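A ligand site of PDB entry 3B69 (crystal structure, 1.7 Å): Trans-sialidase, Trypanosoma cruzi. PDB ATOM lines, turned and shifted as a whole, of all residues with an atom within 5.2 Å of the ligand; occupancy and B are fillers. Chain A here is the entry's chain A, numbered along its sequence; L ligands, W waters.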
ATOM      1  N   ARG A  49      11.828  31.542   4.681  1.00  0.00           N
ATOM      2  CA  ARG A  49      10.399  31.824   4.549  1.00  0.00           C
ATOM      3  C   ARG A  49      10.043  33.128   5.309  1.00  0.00           C
ATOM      4  O   ARG A  49      10.928  33.821   5.815  1.00  0.00           O
ATOM      5  CB  ARG A  49       9.588  30.638   5.122  1.00  0.00           C
ATOM      6  CG  ARG A  49       9.724  29.305   4.407  1.00  0.00           C
ATOM      7  CD  ARG A  49       8.417  28.492   4.613  1.00  0.00           C
ATOM      8  NE  ARG A  49       7.260  29.243   4.143  1.00  0.00           N
ATOM      9  CZ  ARG A  49       5.982  28.876   4.289  1.00  0.00           C
ATOM     10  NH1 ARG A  49       5.015  29.660   3.806  1.00  0.00           N
ATOM     11  NH2 ARG A  49       5.663  27.754   4.920  1.00  0.00           N
ATOM     12  N   LEU A  50       8.752  33.439   5.385  1.00  0.00           N
ATOM     13  CA  LEU A  50       8.288  34.623   6.135  1.00  0.00           C
ATOM     14  C   LEU A  50       8.964  35.940   5.800  1.00  0.00           C
ATOM     15  O   LEU A  50       9.476  36.629   6.696  1.00  0.00           O
ATOM     16  CB  LEU A  50       8.425  34.380   7.650  1.00  0.00           C
ATOM     17  CG  LEU A  50       7.347  33.540   8.357  1.00  0.00           C
ATOM     18  CD1 LEU A  50       6.126  34.435   8.642  1.00  0.00           C
ATOM     19  CD2 LEU A  50       6.944  32.321   7.498  1.00  0.00           C
ATOM     20  N   ASP A  65      12.657  34.050   7.903  1.00  0.00           N
ATOM     21  CA  ASP A  65      12.989  32.861   8.699  1.00  0.00           C
ATOM     22  C   ASP A  65      14.236  32.180   8.069  1.00  0.00           C
ATOM     23  O   ASP A  65      14.340  32.057   6.829  1.00  0.00           O
ATOM     24  CB  ASP A  65      11.871  31.789   8.660  1.00  0.00           C
ATOM     25  CG  ASP A  65      10.747  32.033   9.653  1.00  0.00           C
ATOM     26  OD1 ASP A  65      10.849  32.945  10.492  1.00  0.00           O
ATOM     27  OD2 ASP A  65       9.753  31.296   9.593  1.00  0.00           O
ATOM     28  N   ARG A  67      15.462  28.717   8.241  1.00  0.00           N
ATOM     29  CA  ARG A  67      15.083  27.352   8.651  1.00  0.00           C
ATOM     30  C   ARG A  67      16.276  26.485   8.264  1.00  0.00           C
ATOM     31  O   ARG A  67      16.363  25.949   7.149  1.00  0.00           O
ATOM     32  CB  ARG A  67      13.797  26.924   7.926  1.00  0.00           C
ATOM     33  CG  ARG A  67      12.687  27.924   8.101  1.00  0.00           C
ATOM     34  CD  ARG A  67      11.321  27.352   7.933  1.00  0.00           C
ATOM     35  NE  ARG A  67      10.302  28.351   8.255  1.00  0.00           N
ATOM     36  CZ  ARG A  67       9.000  28.094   8.329  1.00  0.00           C
ATOM     37  NH1 ARG A  67       8.540  26.871   8.092  1.00  0.00           N
ATOM     38  NH2 ARG A  67       8.145  29.074   8.610  1.00  0.00           N
ATOM     39  N   ASP A  73       7.677  23.768   9.828  1.00  0.00           N
ATOM     40  CA  ASP A  73       7.530  24.896  10.747  1.00  0.00           C
ATOM     41  C   ASP A  73       8.214  24.686  12.093  1.00  0.00           C
ATOM     42  O   ASP A  73       8.866  25.573  12.624  1.00  0.00           O
ATOM     43  CB  ASP A  73       6.047  25.171  11.010  1.00  0.00           C
ATOM     44  CG  ASP A  73       5.349  25.762   9.816  1.00  0.00           C
ATOM     45  OD1 ASP A  73       4.103  25.617   9.715  1.00  0.00           O
ATOM     46  OD2 ASP A  73       6.025  26.392   8.977  1.00  0.00           O
ATOM     47  N   VAL A 109       9.905  32.425  15.612  1.00  0.00           N
ATOM     48  CA  VAL A 109       9.002  32.333  14.475  1.00  0.00           C
ATOM     49  C   VAL A 109       8.142  33.525  14.037  1.00  0.00           C
ATOM     50  O   VAL A 109       7.778  34.401  14.832  1.00  0.00           O
ATOM     51  CB  VAL A 109       8.032  31.149  14.725  1.00  0.00           C
ATOM     52  CG1 VAL A 109       8.805  29.884  15.025  1.00  0.00           C
ATOM     53  CG2 VAL A 109       7.101  31.494  15.901  1.00  0.00           C
ATOM     54  N   ASP A 110       7.735  33.449  12.772  1.00  0.00           N
ATOM     55  CA  ASP A 110       6.863  34.421  12.122  1.00  0.00           C
ATOM     56  C   ASP A 110       7.173  35.855  12.505  1.00  0.00           C
ATOM     57  O   ASP A 110       6.323  36.568  13.028  1.00  0.00           O
ATOM     58  CB  ASP A 110       5.399  34.067  12.421  1.00  0.00           C
ATOM     59  CG  ASP A 110       4.961  32.733  11.750  1.00  0.00           C
ATOM     60  OD1 ASP A 110       3.784  32.343  11.883  1.00  0.00           O
ATOM     61  OD2 ASP A 110       5.825  32.087  11.092  1.00  0.00           O
ATOM     62  N   TYR A 133       2.425  21.997  15.781  1.00  0.00           N
ATOM     63  CA  TYR A 133       2.035  23.331  15.281  1.00  0.00           C
ATOM     64  C   TYR A 133       1.450  24.137  16.465  1.00  0.00           C
ATOM     65  O   TYR A 133       0.679  23.599  17.245  1.00  0.00           O
ATOM     66  CB  TYR A 133       1.021  23.183  14.114  1.00  0.00           C
ATOM     67  CG  TYR A 133       1.688  22.717  12.826  1.00  0.00           C
ATOM     68  CD1 TYR A 133       2.313  23.630  11.957  1.00  0.00           C
ATOM     69  CD2 TYR A 133       1.722  21.366  12.467  1.00  0.00           C
ATOM     70  CE1 TYR A 133       2.936  23.194  10.793  1.00  0.00           C
ATOM     71  CE2 TYR A 133       2.337  20.942  11.301  1.00  0.00           C
ATOM     72  CZ  TYR A 133       2.940  21.863  10.472  1.00  0.00           C
ATOM     73  OH  TYR A 133       3.548  21.444   9.311  1.00  0.00           O
ATOM     74  N   TRP A 134       1.818  25.406  16.591  1.00  0.00           N
ATOM     75  CA  TRP A 134       1.368  26.214  17.730  1.00  0.00           C
ATOM     76  C   TRP A 134      -0.135  26.182  18.041  1.00  0.00           C
ATOM     77  O   TRP A 134      -0.502  26.174  19.217  1.00  0.00           O
ATOM     78  CB  TRP A 134       1.861  27.667  17.579  1.00  0.00           C
ATOM     79  CG  TRP A 134       1.065  28.577  16.665  1.00  0.00           C
ATOM     80  CD1 TRP A 134       1.011  28.570  15.275  1.00  0.00           C
ATOM     81  CD2 TRP A 134       0.198  29.643  17.086  1.00  0.00           C
ATOM     82  NE1 TRP A 134       0.157  29.580  14.830  1.00  0.00           N
ATOM     83  CE2 TRP A 134      -0.345  30.249  15.921  1.00  0.00           C
ATOM     84  CE3 TRP A 134      -0.180  30.152  18.356  1.00  0.00           C
ATOM     85  CZ2 TRP A 134      -1.236  31.321  15.992  1.00  0.00           C
ATOM     86  CZ3 TRP A 134      -1.079  31.226  18.414  1.00  0.00           C
ATOM     87  CH2 TRP A 134      -1.585  31.788  17.244  1.00  0.00           C
ATOM     88  N   THR A 135      -0.968  26.097  17.015  1.00  0.00           N
ATOM     89  CA  THR A 135      -2.421  26.105  17.206  1.00  0.00           C
ATOM     90  C   THR A 135      -3.010  24.822  17.771  1.00  0.00           C
ATOM     91  O   THR A 135      -4.180  24.768  18.125  1.00  0.00           O
ATOM     92  CB  THR A 135      -3.160  26.448  15.919  1.00  0.00           C
ATOM     93  OG1 THR A 135      -2.681  25.617  14.858  1.00  0.00           O
ATOM     94  CG2 THR A 135      -2.933  27.899  15.549  1.00  0.00           C
ATOM     95  N   LEU A 190       0.881  35.373  18.594  1.00  0.00           N
ATOM     96  CA  LEU A 190       2.016  35.615  17.733  1.00  0.00           C
ATOM     97  C   LEU A 190       1.711  36.835  16.911  1.00  0.00           C
ATOM     98  O   LEU A 190       0.559  37.258  16.853  1.00  0.00           O
ATOM     99  CB  LEU A 190       2.214  34.424  16.788  1.00  0.00           C
ATOM    100  CG  LEU A 190       2.625  33.070  17.354  1.00  0.00           C
ATOM    101  CD1 LEU A 190       2.699  32.103  16.152  1.00  0.00           C
ATOM    102  CD2 LEU A 190       3.965  33.160  18.063  1.00  0.00           C
ATOM    103  N   GLN A 209      -2.339  37.234  16.135  1.00  0.00           N
ATOM    104  CA  GLN A 209      -3.243  36.087  16.097  1.00  0.00           C
ATOM    105  C   GLN A 209      -3.027  35.444  17.452  1.00  0.00           C
ATOM    106  O   GLN A 209      -1.887  35.239  17.885  1.00  0.00           O
ATOM    107  CB  GLN A 209      -2.894  35.130  14.945  1.00  0.00           C
ATOM    108  CG  GLN A 209      -1.458  34.704  14.903  1.00  0.00           C
ATOM    109  CD  GLN A 209      -1.083  34.101  13.575  1.00  0.00           C
ATOM    110  OE1 GLN A 209       0.050  34.238  13.134  1.00  0.00           O
ATOM    111  NE2 GLN A 209      -2.016  33.435  12.937  1.00  0.00           N
ATOM    112  N   SER A 243      -6.790  34.261  11.189  1.00  0.00           N
ATOM    113  CA  SER A 243      -5.370  34.179  11.542  1.00  0.00           C
ATOM    114  C   SER A 243      -4.499  35.143  10.724  1.00  0.00           C
ATOM    115  O   SER A 243      -5.029  35.884   9.886  1.00  0.00           O
ATOM    116  CB  SER A 243      -4.868  32.738  11.341  1.00  0.00           C
ATOM    117  OG  SER A 243      -4.924  32.347   9.974  1.00  0.00           O
ATOM    118  N   GLU A 244      -3.194  35.145  10.994  1.00  0.00           N
ATOM    119  CA  GLU A 244      -2.222  35.996  10.302  1.00  0.00           C
ATOM    120  C   GLU A 244      -2.803  37.324   9.829  1.00  0.00           C
ATOM    121  O   GLU A 244      -2.751  37.686   8.634  1.00  0.00           O
ATOM    122  CB  GLU A 244      -1.596  35.242   9.129  1.00  0.00           C
ATOM    123  CG  GLU A 244      -0.792  34.047   9.549  1.00  0.00           C
ATOM    124  CD  GLU A 244       0.038  33.520   8.428  1.00  0.00           C
ATOM    125  OE1 GLU A 244      -0.491  33.459   7.287  1.00  0.00           O
ATOM    126  OE2 GLU A 244       1.214  33.162   8.677  1.00  0.00           O
ATOM    127  N   ARG A 259      -6.483  36.300   7.311  1.00  0.00           N
ATOM    128  CA  ARG A 259      -6.413  35.031   6.641  1.00  0.00           C
ATOM    129  C   ARG A 259      -7.489  34.144   7.295  1.00  0.00           C
ATOM    130  O   ARG A 259      -7.594  34.081   8.523  1.00  0.00           O
ATOM    131  CB  ARG A 259      -5.044  34.418   6.842  1.00  0.00           C
ATOM    132  CG  ARG A 259      -4.950  32.951   6.457  1.00  0.00           C
ATOM    133  CD  ARG A 259      -3.528  32.426   6.695  1.00  0.00           C
ATOM    134  NE  ARG A 259      -3.444  31.002   6.433  1.00  0.00           N
ATOM    135  CZ  ARG A 259      -2.311  30.299   6.420  1.00  0.00           C
ATOM    136  NH1 ARG A 259      -1.137  30.885   6.653  1.00  0.00           N
ATOM    137  NH2 ARG A 259      -2.358  28.994   6.159  1.00  0.00           N
ATOM    138  N   ASP A 261      -8.576  30.270   6.771  1.00  0.00           N
ATOM    139  CA  ASP A 261      -8.371  29.011   6.049  1.00  0.00           C
ATOM    140  C   ASP A 261      -9.663  28.425   5.611  1.00  0.00           C
ATOM    141  O   ASP A 261     -10.589  28.321   6.411  1.00  0.00           O
ATOM    142  CB  ASP A 261      -7.614  28.004   6.916  1.00  0.00           C
ATOM    143  CG  ASP A 261      -6.147  28.336   7.010  1.00  0.00           C
ATOM    144  OD1 ASP A 261      -5.500  27.899   7.957  1.00  0.00           O
ATOM    145  OD2 ASP A 261      -5.641  29.035   6.101  1.00  0.00           O
ATOM    146  N   GLY A 298      -5.602  29.511   3.351  1.00  0.00           N
ATOM    147  CA  GLY A 298      -5.243  30.842   2.904  1.00  0.00           C
ATOM    148  C   GLY A 298      -3.746  31.114   3.035  1.00  0.00           C
ATOM    149  O   GLY A 298      -2.931  30.176   3.069  1.00  0.00           O
ATOM    150  N   TRP A 326      -1.686  23.749   0.199  1.00  0.00           N
ATOM    151  CA  TRP A 326      -0.792  24.862   0.526  1.00  0.00           C
ATOM    152  C   TRP A 326       0.142  25.291  -0.570  1.00  0.00           C
ATOM    153  O   TRP A 326       0.924  26.216  -0.373  1.00  0.00           O
ATOM    154  CB  TRP A 326       0.045  24.549   1.770  1.00  0.00           C
ATOM    155  CG  TRP A 326      -0.708  24.602   3.066  1.00  0.00           C
ATOM    156  CD1 TRP A 326      -1.029  25.723   3.803  1.00  0.00           C
ATOM    157  CD2 TRP A 326      -1.297  23.509   3.736  1.00  0.00           C
ATOM    158  NE1 TRP A 326      -1.781  25.379   4.885  1.00  0.00           N
ATOM    159  CE2 TRP A 326      -1.971  24.017   4.862  1.00  0.00           C
ATOM    160  CE3 TRP A 326      -1.328  22.125   3.490  1.00  0.00           C
ATOM    161  CZ2 TRP A 326      -2.670  23.194   5.741  1.00  0.00           C
ATOM    162  CZ3 TRP A 326      -2.013  21.317   4.357  1.00  0.00           C
ATOM    163  CH2 TRP A 326      -2.673  21.849   5.480  1.00  0.00           C
ATOM    164  N   ARG A 328      -0.248  26.982  -3.207  1.00  0.00           N
ATOM    165  CA  ARG A 328      -0.461  28.409  -3.401  1.00  0.00           C
ATOM    166  C   ARG A 328       0.401  29.059  -4.461  1.00  0.00           C
ATOM    167  O   ARG A 328       1.285  29.869  -4.213  1.00  0.00           O
ATOM    168  CB  ARG A 328      -0.331  29.127  -2.061  1.00  0.00           C
ATOM    169  CG  ARG A 328      -1.425  28.697  -1.096  1.00  0.00           C
ATOM    170  CD  ARG A 328      -1.128  29.053   0.332  1.00  0.00           C
ATOM    171  NE  ARG A 328       0.067  28.409   0.859  1.00  0.00           N
ATOM    172  CZ  ARG A 328       0.467  28.473   2.126  1.00  0.00           C
ATOM    173  NH1 ARG A 328      -0.245  29.146   3.033  1.00  0.00           N
ATOM    174  NH2 ARG A 328       1.593  27.866   2.503  1.00  0.00           N
ATOM    175  N   TYR A 356       3.761  33.283   0.833  1.00  0.00           N
ATOM    176  CA  TYR A 356       4.003  34.485   1.616  1.00  0.00           C
ATOM    177  C   TYR A 356       4.809  35.498   0.779  1.00  0.00           C
ATOM    178  O   TYR A 356       5.645  35.113  -0.051  1.00  0.00           O
ATOM    179  CB  TYR A 356       4.727  34.119   2.923  1.00  0.00           C
ATOM    180  CG  TYR A 356       3.920  33.316   3.961  1.00  0.00           C
ATOM    181  CD1 TYR A 356       2.906  32.424   3.582  1.00  0.00           C
ATOM    182  CD2 TYR A 356       4.233  33.397   5.323  1.00  0.00           C
ATOM    183  CE1 TYR A 356       2.225  31.648   4.543  1.00  0.00           C
ATOM    184  CE2 TYR A 356       3.552  32.638   6.288  1.00  0.00           C
ATOM    185  CZ  TYR A 356       2.552  31.754   5.903  1.00  0.00           C
ATOM    186  OH  TYR A 356       1.928  30.977   6.906  1.00  0.00           O
HETATM  187  C1  LIG L   1       1.881  28.867   5.818  1.00  0.00           C
HETATM  188  F1  LIG L   1       4.141  28.148   7.489  1.00  0.00           F
HETATM  189  C2  LIG L   1       2.252  29.634   7.086  1.00  0.00           C
HETATM  190  C3  LIG L   1       3.738  29.480   7.477  1.00  0.00           C
HETATM  191  C4  LIG L   1       3.998  30.093   8.861  1.00  0.00           C
HETATM  192  O1  LIG L   1       5.365  29.912   9.225  1.00  0.00           O
HETATM  193  C5  LIG L   1       3.110  29.380   9.882  1.00  0.00           C
HETATM  194  N1  LIG L   1       3.324  29.917  11.228  1.00  0.00           N
HETATM  195  C6  LIG L   1       1.640  29.496   9.449  1.00  0.00           C
HETATM  196  O2  LIG L   1       1.438  29.035   8.111  1.00  0.00           O
HETATM  197  C7  LIG L   1       0.808  28.604  10.375  1.00  0.00           C
HETATM  198  O3  LIG L   1       1.352  27.283  10.440  1.00  0.00           O
HETATM  199  C8  LIG L   1      -0.640  28.516   9.880  1.00  0.00           C
HETATM  200  O4  LIG L   1      -1.263  29.792  10.035  1.00  0.00           O
HETATM  201  C9  LIG L   1      -1.366  27.458  10.695  1.00  0.00           C
HETATM  202  N2  LIG L   1      -1.124  26.187  10.405  1.00  0.00           N
HETATM  203  C10 LIG L   1       3.413  29.151  12.317  1.00  0.00           C
HETATM  204  O5  LIG L   1       3.297  27.921  12.319  1.00  0.00           O
HETATM  205  C11 LIG L   1       3.642  29.917  13.618  1.00  0.00           C
HETATM  206  C12 LIG L   1      -2.114  25.308  10.321  1.00  0.00           C
HETATM  207  O6  LIG L   1      -3.300  25.576  10.526  1.00  0.00           O
HETATM  208  C13 LIG L   1      -1.682  23.885   9.949  1.00  0.00           C
HETATM  209  C14 LIG L   1      -2.638  22.931   9.590  1.00  0.00           C
HETATM  210  C15 LIG L   1      -2.239  21.681   9.154  1.00  0.00           C
HETATM  211  C16 LIG L   1      -0.890  21.362   9.069  1.00  0.00           C
HETATM  212  C17 LIG L   1       0.066  22.315   9.429  1.00  0.00           C
HETATM  213  C18 LIG L   1      -0.334  23.575   9.874  1.00  0.00           C
HETATM  214  O7  LIG L   1       0.675  28.619   5.631  1.00  0.00           O
HETATM  215  O8  LIG L   1       2.787  28.506   5.027  1.00  0.00           O
HETATM  216  O   HOH W   1      -3.637  29.883   9.550  1.00  0.00           O
HETATM  217  O   HOH W   2      -0.562  31.135  12.274  1.00  0.00           O
HETATM  218  O   HOH W   3       3.878  26.007  14.393  1.00  0.00           O
HETATM  219  O   HOH W   4      -4.339  26.462  12.821  1.00  0.00           O
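The guanidinium group of Arg 67 lies within hydrogen-bond range of an oxygen (O1) of the ligand (3.0 Å). The side-chain hydroxyl of Tyr 356 is covalently linked to a carbon (C2) of the ligand, 1.4 Å away. NH1 of Arg 49 lies within salt-bridge range of O8 of the ligand (2.8 Å). An oxygen (O7) of the ligand lies within salt-bridge range of the guanidinium group (NH1) of Arg 259, at 3.1 Å. The guanidinium group (NH1) of Arg 328 is in salt-bridge range of an oxygen (O7) of the ligand (2.8 Å). The side-chain carboxylate of Asp 73 lies within hydrogen-bond range of an oxygen (O3) of the ligand, at 3.3 Å. N1 of the ligand lies within hydrogen-bond range of OD1 of Asp 110 (2.6 Å).
The guanidinium group (NH2) of Arg 259 lies within hydrogen-bond range of the backbone carbonyl oxygen (O) of Gly 298, 3.4 Å away. The backbone carbonyl oxygen (O) of Arg 49 lies within hydrogen-bond range of the backbone NH (N) of Asp 65 (2.7 Å). The guanidinium group (NH1) of Arg 259 lies within salt-bridge range of the side-chain carboxylate (OE1) of Glu 244 (2.7 Å). The backbone NH (N) of Ser 243 is in hydrogen-bond range of the backbone carbonyl oxygen (O) of Arg 259, 2.8 Å away. The side-chain hydroxyl (OH) of Tyr 356 lies within hydrogen-bond range of the guanidinium group (NH1) of Arg 259, at 3.1 Å. The guanidinium group of Arg 67 is in salt-bridge range of the side-chain carboxylate of Asp 65. N of Glu 244 lies close to NE2 of Gln 209 (2.8 Å). O of Trp 326 is in hydrogen-bond range of NE of Arg 328.
Residues that only touch the ligand: Leu 50, Tyr 133, Trp 134, Leu 190, Glu 244 and Trp 326. The nearest printed residue that does not touch the ligand is Asp 261 (4.1 Å).
Water W1 lies within hydrogen-bond range of an oxygen (O4) of the ligand (2.4 Å), the side-chain hydroxyl (OG) of Ser 243 (2.8 Å), the side-chain carboxylate (OD1) of Asp 261 (3.2 Å) and the guanidinium group (NE) of Arg 259 (3.3 Å). Water W4 lies within hydrogen-bond range of an oxygen (O6) of the ligand (2.7 Å) and the side-chain hydroxyl of Thr 135 (2.8 Å). Water W2 lies within hydrogen-bond range of O4 of the ligand (2.7 Å), NE2 of Gln 209 (2.8 Å) and NE1 of Trp 134 (3.1 Å). Water W3 lies within hydrogen-bond range of O5 of the ligand (2.9 Å) and N of Trp 134 (3.1 Å).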
